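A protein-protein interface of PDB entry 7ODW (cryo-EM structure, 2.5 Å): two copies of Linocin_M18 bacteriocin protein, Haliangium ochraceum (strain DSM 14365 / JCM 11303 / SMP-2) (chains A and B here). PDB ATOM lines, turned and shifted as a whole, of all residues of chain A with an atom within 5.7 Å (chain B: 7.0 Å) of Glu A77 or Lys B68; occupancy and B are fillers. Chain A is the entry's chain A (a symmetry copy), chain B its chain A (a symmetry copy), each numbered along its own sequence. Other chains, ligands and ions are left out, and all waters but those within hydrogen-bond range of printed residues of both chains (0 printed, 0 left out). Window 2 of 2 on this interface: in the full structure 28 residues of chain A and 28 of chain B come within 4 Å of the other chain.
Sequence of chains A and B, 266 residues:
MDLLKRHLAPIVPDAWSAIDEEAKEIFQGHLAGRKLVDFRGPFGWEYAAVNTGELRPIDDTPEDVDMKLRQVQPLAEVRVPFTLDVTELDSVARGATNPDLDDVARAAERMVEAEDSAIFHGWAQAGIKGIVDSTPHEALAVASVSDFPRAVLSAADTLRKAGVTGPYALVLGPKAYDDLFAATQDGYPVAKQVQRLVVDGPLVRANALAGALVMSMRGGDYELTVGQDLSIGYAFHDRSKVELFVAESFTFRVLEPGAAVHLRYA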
ATOM      1  N   TRP A  45      19.153 -19.053 -32.649  1.00  0.00           N
ATOM      2  CA  TRP A  45      19.608 -19.812 -31.495  1.00  0.00           C
ATOM      3  C   TRP A  45      19.519 -19.026 -30.199  1.00  0.00           C
ATOM      4  O   TRP A  45      19.245 -19.612 -29.148  1.00  0.00           O
ATOM      5  CB  TRP A  45      21.046 -20.270 -31.706  1.00  0.00           C
ATOM      6  CG  TRP A  45      21.186 -21.409 -32.635  1.00  0.00           C
ATOM      7  CD1 TRP A  45      21.549 -21.359 -33.942  1.00  0.00           C
ATOM      8  CD2 TRP A  45      20.972 -22.783 -32.329  1.00  0.00           C
ATOM      9  NE1 TRP A  45      21.578 -22.620 -34.472  1.00  0.00           N
ATOM     10  CE2 TRP A  45      21.227 -23.513 -33.498  1.00  0.00           C
ATOM     11  CE3 TRP A  45      20.591 -23.467 -31.178  1.00  0.00           C
ATOM     12  CZ2 TRP A  45      21.112 -24.891 -33.551  1.00  0.00           C
ATOM     13  CZ3 TRP A  45      20.478 -24.832 -31.232  1.00  0.00           C
ATOM     14  CH2 TRP A  45      20.736 -25.532 -32.408  1.00  0.00           C
ATOM     15  N   LEU A  75      11.847 -20.982 -23.802  1.00  0.00           N
ATOM     16  CA  LEU A  75      11.813 -22.008 -24.829  1.00  0.00           C
ATOM     17  C   LEU A  75      12.474 -23.286 -24.335  1.00  0.00           C
ATOM     18  O   LEU A  75      13.273 -23.285 -23.398  1.00  0.00           O
ATOM     19  CB  LEU A  75      12.522 -21.537 -26.092  1.00  0.00           C
ATOM     20  CG  LEU A  75      11.683 -20.858 -27.163  1.00  0.00           C
ATOM     21  CD1 LEU A  75      11.139 -19.559 -26.648  1.00  0.00           C
ATOM     22  CD2 LEU A  75      12.509 -20.623 -28.398  1.00  0.00           C
ATOM     23  N   ALA A  76      12.128 -24.389 -24.980  1.00  0.00           N
ATOM     24  CA  ALA A  76      12.757 -25.671 -24.711  1.00  0.00           C
ATOM     25  C   ALA A  76      13.595 -26.065 -25.914  1.00  0.00           C
ATOM     26  O   ALA A  76      13.132 -25.976 -27.054  1.00  0.00           O
ATOM     27  CB  ALA A  76      11.719 -26.748 -24.413  1.00  0.00           C
ATOM     28  N   GLU A  77      14.830 -26.472 -25.658  1.00  0.00           N
ATOM     29  CA  GLU A  77      15.731 -26.951 -26.693  1.00  0.00           C
ATOM     30  C   GLU A  77      15.813 -28.463 -26.582  1.00  0.00           C
ATOM     31  O   GLU A  77      16.155 -28.993 -25.522  1.00  0.00           O
ATOM     32  CB  GLU A  77      17.114 -26.325 -26.547  1.00  0.00           C
ATOM     33  CG  GLU A  77      18.195 -27.070 -27.288  1.00  0.00           C
ATOM     34  CD  GLU A  77      19.101 -26.151 -28.069  1.00  0.00           C
ATOM     35  OE1 GLU A  77      18.749 -24.967 -28.232  1.00  0.00           O
ATOM     36  OE2 GLU A  77      20.170 -26.609 -28.517  1.00  0.00           O
ATOM     37  N   VAL A  78      15.491 -29.154 -27.668  1.00  0.00           N
ATOM     38  CA  VAL A  78      15.393 -30.604 -27.671  1.00  0.00           C
ATOM     39  C   VAL A  78      16.273 -31.150 -28.784  1.00  0.00           C
ATOM     40  O   VAL A  78      16.255 -30.642 -29.913  1.00  0.00           O
ATOM     41  CB  VAL A  78      13.933 -31.069 -27.825  1.00  0.00           C
ATOM     42  CG1 VAL A  78      13.297 -30.432 -29.034  1.00  0.00           C
ATOM     43  CG2 VAL A  78      13.865 -32.574 -27.913  1.00  0.00           C
ATOM     44  N   ARG A  79      17.063 -32.165 -28.446  1.00  0.00           N
ATOM     45  CA  ARG A  79      17.947 -32.850 -29.378  1.00  0.00           C
ATOM     46  C   ARG A  79      17.675 -34.337 -29.281  1.00  0.00           C
ATOM     47  O   ARG A  79      17.681 -34.899 -28.184  1.00  0.00           O
ATOM     48  CB  ARG A  79      19.413 -32.575 -29.054  1.00  0.00           C
ATOM     49  CG  ARG A  79      19.953 -31.309 -29.633  1.00  0.00           C
ATOM     50  CD  ARG A  79      21.274 -30.985 -28.998  1.00  0.00           C
ATOM     51  NE  ARG A  79      21.711 -29.642 -29.342  1.00  0.00           N
ATOM     52  CZ  ARG A  79      22.972 -29.316 -29.574  1.00  0.00           C
ATOM     53  NH1 ARG A  79      23.914 -30.240 -29.494  1.00  0.00           N
ATOM     54  NH2 ARG A  79      23.289 -28.071 -29.884  1.00  0.00           N
ATOM     55  N   ALA A 247      17.721 -31.248 -33.937  1.00  0.00           N
ATOM     56  CA  ALA A 247      17.674 -30.224 -32.910  1.00  0.00           C
ATOM     57  C   ALA A 247      16.590 -29.214 -33.229  1.00  0.00           C
ATOM     58  O   ALA A 247      16.386 -28.853 -34.394  1.00  0.00           O
ATOM     59  CB  ALA A 247      19.012 -29.506 -32.780  1.00  0.00           C
ATOM     60  N   GLU A 248      15.901 -28.760 -32.184  1.00  0.00           N
ATOM     61  CA  GLU A 248      14.885 -27.729 -32.335  1.00  0.00           C
ATOM     62  C   GLU A 248      14.668 -27.016 -31.011  1.00  0.00           C
ATOM     63  O   GLU A 248      14.635 -27.651 -29.958  1.00  0.00           O
ATOM     64  CB  GLU A 248      13.565 -28.321 -32.822  1.00  0.00           C
ATOM     65  CG  GLU A 248      12.717 -27.355 -33.607  1.00  0.00           C
ATOM     66  CD  GLU A 248      11.242 -27.645 -33.463  1.00  0.00           C
ATOM     67  OE1 GLU A 248      10.453 -27.150 -34.294  1.00  0.00           O
ATOM     68  OE2 GLU A 248      10.873 -28.372 -32.519  1.00  0.00           O
ATOM     69  N   SER A 249      14.500 -25.699 -31.075  1.00  0.00           N
ATOM     70  CA  SER A 249      14.166 -24.889 -29.910  1.00  0.00           C
ATOM     71  C   SER A 249      12.795 -24.276 -30.137  1.00  0.00           C
ATOM     72  O   SER A 249      12.606 -23.512 -31.088  1.00  0.00           O
ATOM     73  CB  SER A 249      15.205 -23.799 -29.677  1.00  0.00           C
ATOM     74  OG  SER A 249      15.068 -22.780 -30.647  1.00  0.00           O
ATOM     75  N   PHE A 250      11.852 -24.594 -29.260  1.00  0.00           N
ATOM     76  CA  PHE A 250      10.472 -24.200 -29.484  1.00  0.00           C
ATOM     77  C   PHE A 250       9.740 -24.066 -28.161  1.00  0.00           C
ATOM     78  O   PHE A 250      10.169 -24.586 -27.130  1.00  0.00           O
ATOM     79  CB  PHE A 250       9.739 -25.216 -30.365  1.00  0.00           C
ATOM     80  CG  PHE A 250       9.260 -26.413 -29.611  1.00  0.00           C
ATOM     81  CD1 PHE A 250      10.134 -27.415 -29.264  1.00  0.00           C
ATOM     82  CD2 PHE A 250       7.943 -26.526 -29.228  1.00  0.00           C
ATOM     83  CE1 PHE A 250       9.704 -28.508 -28.561  1.00  0.00           C
ATOM     84  CE2 PHE A 250       7.512 -27.617 -28.522  1.00  0.00           C
ATOM     85  CZ  PHE A 250       8.394 -28.609 -28.190  1.00  0.00           C
ATOM     86  N   LEU B  55      21.647 -23.020 -20.367  1.00  0.00           N
ATOM     87  CA  LEU B  55      20.639 -24.054 -20.494  1.00  0.00           C
ATOM     88  C   LEU B  55      20.591 -24.845 -19.202  1.00  0.00           C
ATOM     89  O   LEU B  55      21.607 -25.026 -18.530  1.00  0.00           O
ATOM     90  CB  LEU B  55      20.940 -24.987 -21.655  1.00  0.00           C
ATOM     91  CG  LEU B  55      20.633 -24.436 -23.039  1.00  0.00           C
ATOM     92  CD1 LEU B  55      21.456 -25.148 -24.079  1.00  0.00           C
ATOM     93  CD2 LEU B  55      19.172 -24.619 -23.322  1.00  0.00           C
ATOM     94  N   ARG B  56      19.405 -25.311 -18.857  1.00  0.00           N
ATOM     95  CA  ARG B  56      19.215 -26.102 -17.670  1.00  0.00           C
ATOM     96  C   ARG B  56      18.750 -27.495 -18.059  1.00  0.00           C
ATOM     97  O   ARG B  56      17.828 -27.633 -18.868  1.00  0.00           O
ATOM     98  CB  ARG B  56      18.184 -25.456 -16.740  1.00  0.00           C
ATOM     99  CG  ARG B  56      18.253 -25.927 -15.306  1.00  0.00           C
ATOM    100  CD  ARG B  56      19.504 -25.422 -14.613  1.00  0.00           C
ATOM    101  NE  ARG B  56      19.824 -24.048 -14.985  1.00  0.00           N
ATOM    102  CZ  ARG B  56      21.056 -23.601 -15.203  1.00  0.00           C
ATOM    103  NH1 ARG B  56      22.091 -24.421 -15.087  1.00  0.00           N
ATOM    104  NH2 ARG B  56      21.257 -22.335 -15.536  1.00  0.00           N
ATOM    105  N   PRO B  57      19.370 -28.541 -17.518  1.00  0.00           N
ATOM    106  CA  PRO B  57      18.970 -29.901 -17.882  1.00  0.00           C
ATOM    107  C   PRO B  57      17.658 -30.269 -17.209  1.00  0.00           C
ATOM    108  O   PRO B  57      17.514 -30.152 -15.992  1.00  0.00           O
ATOM    109  CB  PRO B  57      20.122 -30.769 -17.369  1.00  0.00           C
ATOM    110  CG  PRO B  57      20.954 -29.892 -16.497  1.00  0.00           C
ATOM    111  CD  PRO B  57      20.381 -28.520 -16.455  1.00  0.00           C
ATOM    112  N   ILE B  58      16.705 -30.717 -18.010  1.00  0.00           N
ATOM    113  CA  ILE B  58      15.397 -31.115 -17.513  1.00  0.00           C
ATOM    114  C   ILE B  58      15.469 -32.564 -17.068  1.00  0.00           C
ATOM    115  O   ILE B  58      15.919 -33.435 -17.820  1.00  0.00           O
ATOM    116  CB  ILE B  58      14.322 -30.924 -18.590  1.00  0.00           C
ATOM    117  CG1 ILE B  58      14.171 -29.447 -18.930  1.00  0.00           C
ATOM    118  CG2 ILE B  58      13.007 -31.482 -18.119  1.00  0.00           C
ATOM    119  CD1 ILE B  58      13.465 -29.209 -20.232  1.00  0.00           C
ATOM    120  N   THR B  61      13.369 -37.294 -18.461  1.00  0.00           N
ATOM    121  CA  THR B  61      13.206 -37.207 -19.899  1.00  0.00           C
ATOM    122  C   THR B  61      13.570 -38.542 -20.531  1.00  0.00           C
ATOM    123  O   THR B  61      14.406 -39.280 -19.998  1.00  0.00           O
ATOM    124  CB  THR B  61      14.076 -36.078 -20.479  1.00  0.00           C
ATOM    125  OG1 THR B  61      13.610 -35.720 -21.785  1.00  0.00           O
ATOM    126  CG2 THR B  61      15.539 -36.483 -20.547  1.00  0.00           C
ATOM    127  N   VAL B  65      15.462 -38.745 -26.475  1.00  0.00           N
ATOM    128  CA  VAL B  65      15.385 -37.296 -26.602  1.00  0.00           C
ATOM    129  C   VAL B  65      16.220 -36.667 -25.499  1.00  0.00           C
ATOM    130  O   VAL B  65      16.273 -37.186 -24.381  1.00  0.00           O
ATOM    131  CB  VAL B  65      13.931 -36.794 -26.530  1.00  0.00           C
ATOM    132  CG1 VAL B  65      13.874 -35.300 -26.748  1.00  0.00           C
ATOM    133  CG2 VAL B  65      13.075 -37.501 -27.555  1.00  0.00           C
ATOM    134  N   ASP B  66      16.886 -35.563 -25.818  1.00  0.00           N
ATOM    135  CA  ASP B  66      17.557 -34.731 -24.834  1.00  0.00           C
ATOM    136  C   ASP B  66      16.873 -33.374 -24.800  1.00  0.00           C
ATOM    137  O   ASP B  66      16.753 -32.711 -25.835  1.00  0.00           O
ATOM    138  CB  ASP B  66      19.038 -34.576 -25.162  1.00  0.00           C
ATOM    139  CG  ASP B  66      19.782 -33.790 -24.115  1.00  0.00           C
ATOM    140  OD1 ASP B  66      19.812 -32.548 -24.215  1.00  0.00           O
ATOM    141  OD2 ASP B  66      20.334 -34.412 -23.186  1.00  0.00           O
ATOM    142  N   MET B  67      16.429 -32.964 -23.617  1.00  0.00           N
ATOM    143  CA  MET B  67      15.615 -31.769 -23.462  1.00  0.00           C
ATOM    144  C   MET B  67      16.284 -30.828 -22.476  1.00  0.00           C
ATOM    145  O   MET B  67      16.678 -31.246 -21.385  1.00  0.00           O
ATOM    146  CB  MET B  67      14.204 -32.134 -22.989  1.00  0.00           C
ATOM    147  CG  MET B  67      13.115 -31.138 -23.379  1.00  0.00           C
ATOM    148  SD  MET B  67      11.610 -31.311 -22.389  1.00  0.00           S
ATOM    149  CE  MET B  67      10.350 -31.495 -23.652  1.00  0.00           C
ATOM    150  N   LYS B  68      16.419 -29.565 -22.865  1.00  0.00           N
ATOM    151  CA  LYS B  68      17.002 -28.536 -22.019  1.00  0.00           C
ATOM    152  C   LYS B  68      16.131 -27.293 -22.069  1.00  0.00           C
ATOM    153  O   LYS B  68      15.505 -26.998 -23.088  1.00  0.00           O
ATOM    154  CB  LYS B  68      18.418 -28.180 -22.457  1.00  0.00           C
ATOM    155  CG  LYS B  68      19.371 -29.344 -22.476  1.00  0.00           C
ATOM    156  CD  LYS B  68      20.198 -29.386 -21.219  1.00  0.00           C
ATOM    157  CE  LYS B  68      21.531 -30.040 -21.485  1.00  0.00           C
ATOM    158  NZ  LYS B  68      21.994 -29.754 -22.866  1.00  0.00           N
ATOM    159  N   LEU B  69      16.109 -26.557 -20.965  1.00  0.00           N
ATOM    160  CA  LEU B  69      15.289 -25.361 -20.839  1.00  0.00           C
ATOM    161  C   LEU B  69      16.168 -24.123 -20.839  1.00  0.00           C
ATOM    162  O   LEU B  69      17.143 -24.055 -20.091  1.00  0.00           O
ATOM    163  CB  LEU B  69      14.461 -25.412 -19.560  1.00  0.00           C
ATOM    164  CG  LEU B  69      13.030 -24.892 -19.659  1.00  0.00           C
ATOM    165  CD1 LEU B  69      12.447 -25.167 -21.026  1.00  0.00           C
ATOM    166  CD2 LEU B  69      12.182 -25.525 -18.585  1.00  0.00           C
ATOM    167  N   ARG B  70      15.821 -23.147 -21.665  1.00  0.00           N
ATOM    168  CA  ARG B  70      16.566 -21.900 -21.678  1.00  0.00           C
ATOM    169  C   ARG B  70      16.406 -21.174 -20.351  1.00  0.00           C
ATOM    170  O   ARG B  70      15.407 -21.331 -19.649  1.00  0.00           O
ATOM    171  CB  ARG B  70      16.100 -21.010 -22.820  1.00  0.00           C
ATOM    172  CG  ARG B  70      16.574 -21.458 -24.178  1.00  0.00           C
ATOM    173  CD  ARG B  70      18.074 -21.374 -24.286  1.00  0.00           C
ATOM    174  NE  ARG B  70      18.529 -20.027 -24.588  1.00  0.00           N
ATOM    175  CZ  ARG B  70      18.731 -19.576 -25.816  1.00  0.00           C
ATOM    176  NH1 ARG B  70      18.515 -20.367 -26.850  1.00  0.00           N
ATOM    177  NH2 ARG B  70      19.146 -18.338 -26.011  1.00  0.00           N
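N of Asp B66 lies within hydrogen-bond range of O of Arg A79 (2.6 Å). The backbone NH (N) of Glu A77 lies within hydrogen-bond range of the backbone carbonyl oxygen (O) of Lys B68, at 2.7 Å. The backbone carbonyl oxygen of Trp A45 sits at hydrogen-bond distance from the guanidinium group of Arg B70, 2.5 Å away. The backbone NH of Arg B70 sits at hydrogen-bond distance from the backbone carbonyl oxygen of Leu A75 (3.1 Å).
N of Arg B56 is in hydrogen-bond range of O of Leu B69 (2.9 Å). N of Ile B58 is in hydrogen-bond range of O of Met B67 (3.4 Å). OD1 of Asp B66 is in salt-bridge range of NZ of Lys B68 (3.8 Å). The backbone NH (N) of Phe A250 sits at hydrogen-bond distance from the backbone carbonyl oxygen (O) of Ala A76 (2.9 Å). The guanidinium group (NE) of Arg A79 lies within salt-bridge range of the side-chain carboxylate (OE2) of Glu A77 (3.5 Å). The backbone NH (N) of Val A78 is in hydrogen-bond range of the backbone carbonyl oxygen (O) of Glu A248.
Leu A75 touches Leu B69 (O to CD1, 3.1 Å). Lys B68 touches Ala A76. CD1 of Leu B69 touches CA of Ala A76, 3.7 Å away. Glu A77 touches Asp B66. Met B67 touches Glu A77. CG2 of Val A78 touches CG1 of Val B65, at 3.0 Å. Asp B66 touches Val A78. Val B65 touches Arg A79 (C to O, 3.5 Å).
Glu A77 touches three residues of chain B. Of the printed residues of chain B, Ala A76 touches Lys B68 and Leu B69. Of the printed residues of chain A, Met B67 touches Glu A77. Ser A249 touches none of the printed residues of chain B.
Hydrophobic or aromatic side chains of chain A that line the printed part of chain B: Ala A76 and Val A78. Printed residues of chain B that touch a printed residue of chain A: Val B65, Asp B66, Met B67, Lys B68, Leu B69 and Arg B70. Along chain B the printed residues that touch a printed residue of chain A span positions 65 to 70. Among the printed residues, no Asp or Glu carboxylate lies within 4 Å of a Lys or Arg side-chain nitrogen of the other chain.
No position is printed for both chains. Of the 12 pairs that touch across the chains among the printed residues, none has its exchanged pair printed and touching as well.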
